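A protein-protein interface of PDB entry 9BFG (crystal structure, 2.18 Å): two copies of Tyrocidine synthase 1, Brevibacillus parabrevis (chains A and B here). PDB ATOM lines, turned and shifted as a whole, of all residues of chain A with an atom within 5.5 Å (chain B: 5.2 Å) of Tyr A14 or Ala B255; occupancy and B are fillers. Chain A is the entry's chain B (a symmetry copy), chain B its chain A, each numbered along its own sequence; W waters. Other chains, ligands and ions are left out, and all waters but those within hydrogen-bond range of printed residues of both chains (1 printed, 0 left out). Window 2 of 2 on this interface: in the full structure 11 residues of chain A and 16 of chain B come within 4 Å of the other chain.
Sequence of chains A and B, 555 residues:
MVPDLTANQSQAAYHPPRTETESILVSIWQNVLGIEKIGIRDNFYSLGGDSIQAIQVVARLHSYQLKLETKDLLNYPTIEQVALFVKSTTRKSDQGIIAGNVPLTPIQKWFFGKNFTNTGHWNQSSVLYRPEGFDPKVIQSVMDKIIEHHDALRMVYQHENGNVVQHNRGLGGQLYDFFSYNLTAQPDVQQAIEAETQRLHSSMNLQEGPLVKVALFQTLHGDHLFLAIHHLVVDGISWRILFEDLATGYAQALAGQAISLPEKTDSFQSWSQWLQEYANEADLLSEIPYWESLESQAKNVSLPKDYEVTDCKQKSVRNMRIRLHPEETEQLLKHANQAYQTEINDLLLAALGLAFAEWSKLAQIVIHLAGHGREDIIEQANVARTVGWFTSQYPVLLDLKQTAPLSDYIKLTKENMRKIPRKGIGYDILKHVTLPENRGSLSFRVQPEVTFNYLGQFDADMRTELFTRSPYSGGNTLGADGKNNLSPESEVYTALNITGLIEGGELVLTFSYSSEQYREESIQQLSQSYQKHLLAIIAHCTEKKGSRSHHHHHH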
ATOM      1  N   ALA A  13      -5.912 -17.073 -12.637  1.00  0.00           N
ATOM      2  CA  ALA A  13      -5.220 -17.618 -13.849  1.00  0.00           C
ATOM      3  C   ALA A  13      -3.760 -17.939 -13.525  1.00  0.00           C
ATOM      4  O   ALA A  13      -3.138 -17.213 -12.743  1.00  0.00           O
ATOM      5  CB  ALA A  13      -5.302 -16.654 -15.010  1.00  0.00           C
ATOM      6  N   TYR A  14      -3.260 -19.005 -14.141  1.00  0.00           N
ATOM      7  CA  TYR A  14      -1.834 -19.394 -14.164  1.00  0.00           C
ATOM      8  C   TYR A  14      -1.102 -18.518 -15.188  1.00  0.00           C
ATOM      9  O   TYR A  14      -1.384 -18.601 -16.400  1.00  0.00           O
ATOM     10  CB  TYR A  14      -1.721 -20.880 -14.514  1.00  0.00           C
ATOM     11  CG  TYR A  14      -0.313 -21.322 -14.792  1.00  0.00           C
ATOM     12  CD1 TYR A  14       0.587 -21.515 -13.768  1.00  0.00           C
ATOM     13  CD2 TYR A  14       0.141 -21.476 -16.085  1.00  0.00           C
ATOM     14  CE1 TYR A  14       1.898 -21.882 -14.019  1.00  0.00           C
ATOM     15  CE2 TYR A  14       1.439 -21.862 -16.356  1.00  0.00           C
ATOM     16  CZ  TYR A  14       2.318 -22.072 -15.318  1.00  0.00           C
ATOM     17  OH  TYR A  14       3.605 -22.427 -15.587  1.00  0.00           O
ATOM     18  N   HIS A  15      -0.143 -17.720 -14.731  1.00  0.00           N
ATOM     19  CA  HIS A  15       0.748 -16.935 -15.621  1.00  0.00           C
ATOM     20  C   HIS A  15       2.087 -17.649 -15.731  1.00  0.00           C
ATOM     21  O   HIS A  15       2.852 -17.714 -14.771  1.00  0.00           O
ATOM     22  CB  HIS A  15       0.865 -15.487 -15.126  1.00  0.00           C
ATOM     23  CG  HIS A  15      -0.458 -14.820 -14.965  1.00  0.00           C
ATOM     24  ND1 HIS A  15      -1.272 -15.039 -13.859  1.00  0.00           N
ATOM     25  CD2 HIS A  15      -1.127 -13.974 -15.767  1.00  0.00           C
ATOM     26  CE1 HIS A  15      -2.380 -14.329 -13.984  1.00  0.00           C
ATOM     27  NE2 HIS A  15      -2.316 -13.676 -15.146  1.00  0.00           N
ATOM     28  N   PRO A  16       2.413 -18.202 -16.914  1.00  0.00           N
ATOM     29  CA  PRO A  16       3.680 -18.888 -17.116  1.00  0.00           C
ATOM     30  C   PRO A  16       4.881 -17.968 -17.057  1.00  0.00           C
ATOM     31  O   PRO A  16       4.746 -16.761 -17.294  1.00  0.00           O
ATOM     32  CB  PRO A  16       3.599 -19.437 -18.548  1.00  0.00           C
ATOM     33  CG  PRO A  16       2.558 -18.580 -19.203  1.00  0.00           C
ATOM     34  CD  PRO A  16       1.561 -18.259 -18.109  1.00  0.00           C
ATOM     35  N   PRO A  17       6.082 -18.531 -16.784  1.00  0.00           N
ATOM     36  CA  PRO A  17       7.316 -17.765 -16.861  1.00  0.00           C
ATOM     37  C   PRO A  17       7.472 -17.296 -18.310  1.00  0.00           C
ATOM     38  O   PRO A  17       6.822 -17.888 -19.143  1.00  0.00           O
ATOM     39  CB  PRO A  17       8.410 -18.749 -16.438  1.00  0.00           C
ATOM     40  CG  PRO A  17       7.790 -20.097 -16.727  1.00  0.00           C
ATOM     41  CD  PRO A  17       6.327 -19.925 -16.391  1.00  0.00           C
ATOM     42  N   VAL A  26      10.452 -20.098 -10.949  1.00  0.00           N
ATOM     43  CA  VAL A  26       9.260 -21.002 -10.834  1.00  0.00           C
ATOM     44  C   VAL A  26       9.707 -22.351 -10.245  1.00  0.00           C
ATOM     45  O   VAL A  26       9.096 -22.871  -9.306  1.00  0.00           O
ATOM     46  CB  VAL A  26       8.563 -21.221 -12.192  1.00  0.00           C
ATOM     47  CG1 VAL A  26       7.624 -22.412 -12.142  1.00  0.00           C
ATOM     48  CG2 VAL A  26       7.817 -19.977 -12.643  1.00  0.00           C
ATOM     49  N   LYS A  37       2.606 -26.508  -9.535  1.00  0.00           N
ATOM     50  CA  LYS A  37       2.581 -25.551 -10.667  1.00  0.00           C
ATOM     51  C   LYS A  37       2.441 -24.164 -10.043  1.00  0.00           C
ATOM     52  O   LYS A  37       1.427 -23.891  -9.392  1.00  0.00           O
ATOM     53  CB  LYS A  37       1.489 -25.931 -11.675  1.00  0.00           C
ATOM     54  N   ILE A  38       3.473 -23.340 -10.149  1.00  0.00           N
ATOM     55  CA  ILE A  38       3.448 -21.968  -9.564  1.00  0.00           C
ATOM     56  C   ILE A  38       3.511 -20.981 -10.729  1.00  0.00           C
ATOM     57  O   ILE A  38       4.366 -21.144 -11.609  1.00  0.00           O
ATOM     58  CB  ILE A  38       4.568 -21.760  -8.510  1.00  0.00           C
ATOM     59  CG1 ILE A  38       4.244 -22.512  -7.208  1.00  0.00           C
ATOM     60  CG2 ILE A  38       4.815 -20.269  -8.267  1.00  0.00           C
ATOM     61  CD1 ILE A  38       5.382 -22.564  -6.191  1.00  0.00           C
ATOM     62  N   GLY A  39       2.609 -20.009 -10.704  1.00  0.00           N
ATOM     63  CA  GLY A  39       2.579 -18.866 -11.634  1.00  0.00           C
ATOM     64  C   GLY A  39       3.384 -17.688 -11.122  1.00  0.00           C
ATOM     65  O   GLY A  39       3.527 -17.551  -9.879  1.00  0.00           O
ATOM     66  N   THR B 248      -0.331 -17.626 -24.053  1.00  0.00           N
ATOM     67  CA  THR B 248      -0.739 -17.845 -22.638  1.00  0.00           C
ATOM     68  C   THR B 248      -1.487 -19.182 -22.533  1.00  0.00           C
ATOM     69  O   THR B 248      -1.106 -20.065 -21.675  1.00  0.00           O
ATOM     70  CB  THR B 248      -1.619 -16.710 -22.111  1.00  0.00           C
ATOM     71  OG1 THR B 248      -0.799 -15.548 -22.139  1.00  0.00           O
ATOM     72  CG2 THR B 248      -2.173 -16.961 -20.721  1.00  0.00           C
ATOM     73  N   TYR B 250      -1.673 -21.726 -24.557  1.00  0.00           N
ATOM     74  CA  TYR B 250      -0.857 -22.888 -24.953  1.00  0.00           C
ATOM     75  C   TYR B 250       0.016 -23.247 -23.758  1.00  0.00           C
ATOM     76  O   TYR B 250       0.057 -24.455 -23.415  1.00  0.00           O
ATOM     77  CB  TYR B 250      -0.068 -22.649 -26.245  1.00  0.00           C
ATOM     78  CG  TYR B 250       0.373 -23.917 -26.937  1.00  0.00           C
ATOM     79  CD1 TYR B 250       1.464 -24.619 -26.494  1.00  0.00           C
ATOM     80  CD2 TYR B 250      -0.313 -24.420 -28.029  1.00  0.00           C
ATOM     81  CE1 TYR B 250       1.872 -25.796 -27.097  1.00  0.00           C
ATOM     82  CE2 TYR B 250       0.069 -25.589 -28.661  1.00  0.00           C
ATOM     83  CZ  TYR B 250       1.179 -26.279 -28.195  1.00  0.00           C
ATOM     84  OH  TYR B 250       1.565 -27.451 -28.762  1.00  0.00           O
ATOM     85  N   ALA B 251       0.689 -22.271 -23.134  1.00  0.00           N
ATOM     86  CA  ALA B 251       1.573 -22.550 -21.967  1.00  0.00           C
ATOM     87  C   ALA B 251       0.731 -23.081 -20.784  1.00  0.00           C
ATOM     88  O   ALA B 251       1.207 -23.969 -20.032  1.00  0.00           O
ATOM     89  CB  ALA B 251       2.373 -21.340 -21.583  1.00  0.00           C
ATOM     90  N   GLN B 252      -0.492 -22.584 -20.620  1.00  0.00           N
ATOM     91  CA  GLN B 252      -1.368 -23.046 -19.519  1.00  0.00           C
ATOM     92  C   GLN B 252      -1.702 -24.532 -19.723  1.00  0.00           C
ATOM     93  O   GLN B 252      -1.484 -25.315 -18.766  1.00  0.00           O
ATOM     94  CB  GLN B 252      -2.628 -22.192 -19.411  1.00  0.00           C
ATOM     95  CG  GLN B 252      -2.356 -20.778 -18.929  1.00  0.00           C
ATOM     96  CD  GLN B 252      -3.516 -19.829 -19.116  1.00  0.00           C
ATOM     97  OE1 GLN B 252      -4.347 -19.983 -19.996  1.00  0.00           O
ATOM     98  NE2 GLN B 252      -3.639 -18.888 -18.199  1.00  0.00           N
ATOM     99  N   ALA B 253      -2.154 -24.930 -20.921  1.00  0.00           N
ATOM    100  CA  ALA B 253      -2.436 -26.346 -21.285  1.00  0.00           C
ATOM    101  C   ALA B 253      -1.195 -27.221 -21.066  1.00  0.00           C
ATOM    102  O   ALA B 253      -1.340 -28.256 -20.396  1.00  0.00           O
ATOM    103  CB  ALA B 253      -2.933 -26.446 -22.700  1.00  0.00           C
ATOM    104  N   LEU B 254      -0.017 -26.803 -21.529  1.00  0.00           N
ATOM    105  CA  LEU B 254       1.252 -27.566 -21.338  1.00  0.00           C
ATOM    106  C   LEU B 254       1.504 -27.806 -19.850  1.00  0.00           C
ATOM    107  O   LEU B 254       1.920 -28.901 -19.526  1.00  0.00           O
ATOM    108  CB  LEU B 254       2.452 -26.830 -21.943  1.00  0.00           C
ATOM    109  CG  LEU B 254       2.624 -26.915 -23.457  1.00  0.00           C
ATOM    110  CD1 LEU B 254       4.081 -26.726 -23.859  1.00  0.00           C
ATOM    111  CD2 LEU B 254       2.093 -28.224 -24.003  1.00  0.00           C
ATOM    112  N   ALA B 255       1.251 -26.823 -18.982  1.00  0.00           N
ATOM    113  CA  ALA B 255       1.489 -26.920 -17.518  1.00  0.00           C
ATOM    114  C   ALA B 255       0.378 -27.708 -16.806  1.00  0.00           C
ATOM    115  O   ALA B 255       0.437 -27.803 -15.567  1.00  0.00           O
ATOM    116  CB  ALA B 255       1.584 -25.532 -16.934  1.00  0.00           C
ATOM    117  N   GLY B 256      -0.651 -28.159 -17.519  1.00  0.00           N
ATOM    118  CA  GLY B 256      -1.795 -28.856 -16.905  1.00  0.00           C
ATOM    119  C   GLY B 256      -2.691 -27.893 -16.153  1.00  0.00           C
ATOM    120  O   GLY B 256      -3.358 -28.326 -15.238  1.00  0.00           O
ATOM    121  N   GLN B 257      -2.728 -26.620 -16.537  1.00  0.00           N
ATOM    122  CA  GLN B 257      -3.547 -25.589 -15.842  1.00  0.00           C
ATOM    123  C   GLN B 257      -4.751 -25.256 -16.711  1.00  0.00           C
ATOM    124  O   GLN B 257      -4.669 -25.454 -17.930  1.00  0.00           O
ATOM    125  CB  GLN B 257      -2.741 -24.314 -15.610  1.00  0.00           C
ATOM    126  CG  GLN B 257      -1.438 -24.564 -14.877  1.00  0.00           C
ATOM    127  CD  GLN B 257      -1.751 -25.159 -13.532  1.00  0.00           C
ATOM    128  OE1 GLN B 257      -1.321 -26.258 -13.210  1.00  0.00           O
ATOM    129  NE2 GLN B 257      -2.571 -24.453 -12.777  1.00  0.00           N
ATOM    130  N   ALA B 258      -5.820 -24.734 -16.123  1.00  0.00           N
ATOM    131  CA  ALA B 258      -6.980 -24.282 -16.914  1.00  0.00           C
ATOM    132  C   ALA B 258      -6.503 -23.177 -17.865  1.00  0.00           C
ATOM    133  O   ALA B 258      -5.651 -22.361 -17.487  1.00  0.00           O
ATOM    134  CB  ALA B 258      -8.101 -23.808 -16.018  1.00  0.00           C
HETATM  135  O   HOH W   1      -4.965 -20.781 -15.118  1.00  0.00           O
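The backbone carbonyl oxygen (O) of Ala B255 lies close to the side-chain amide oxygen (OE1) of Gln B257, 3.3 Å away. The backbone carbonyl oxygen (O) of Gln B252 sits at hydrogen-bond distance from the backbone NH (N) of Gln B257, at 2.9 Å.
Of the printed residues of chain B, Tyr A14 touches Gln B252 (2.9 Å), Ala B255 (3.7 Å) and Gln B257 (3.4 Å). Ala B255 touches just one residue of chain A: Tyr A14 (3.7 Å). Of the printed residues of chain A, Gln B257 touches Tyr A14 and Lys A37. Of the printed residues of chain B, Pro A16 touches Ala B251. The nearest residue of chain B that does not touch Tyr A14 is Ala B251 (4.2 Å). The nearest residue of chain A that does not touch Ala B255 is Lys A37 (4.4 Å). The nearest printed residue of chain A that does not touch Gln B257 is Ile A38 (6.4 Å).
No position is printed for both chains. Of the 5 pairs that touch across the chains among the printed residues, none has its exchanged pair printed and touching as well.
Water W1 lies within hydrogen-bond range of N of Tyr A14 (2.6 Å) and O of Ala B258 (2.9 Å).
Of the 10 printed residues of chain B, 4 touch a printed residue of chain A. Printed residues of chain B that touch a printed residue of chain A: Ala B251, Gln B252, Ala B255 and Gln B257. Hydrophobic or aromatic side chains of chain A within 4 Å of the printed part of chain B: Tyr A14 and Pro A16. Among the printed residues, no Asp or Glu carboxylate lies within 4 Å of a Lys or Arg side-chain nitrogen of the other chain.
The backbone carbonyl oxygen (O) of Tyr A14 sits at hydrogen-bond distance from the side-chain amide nitrogen (NE2) of Gln B252 (2.9 Å).
Among the printed residues, pairs that only touch across the chains: Lys A37 with Gln B257, Tyr A14 with Gln B257, Pro A16 with Ala B251 and Tyr A14 with Ala B255.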
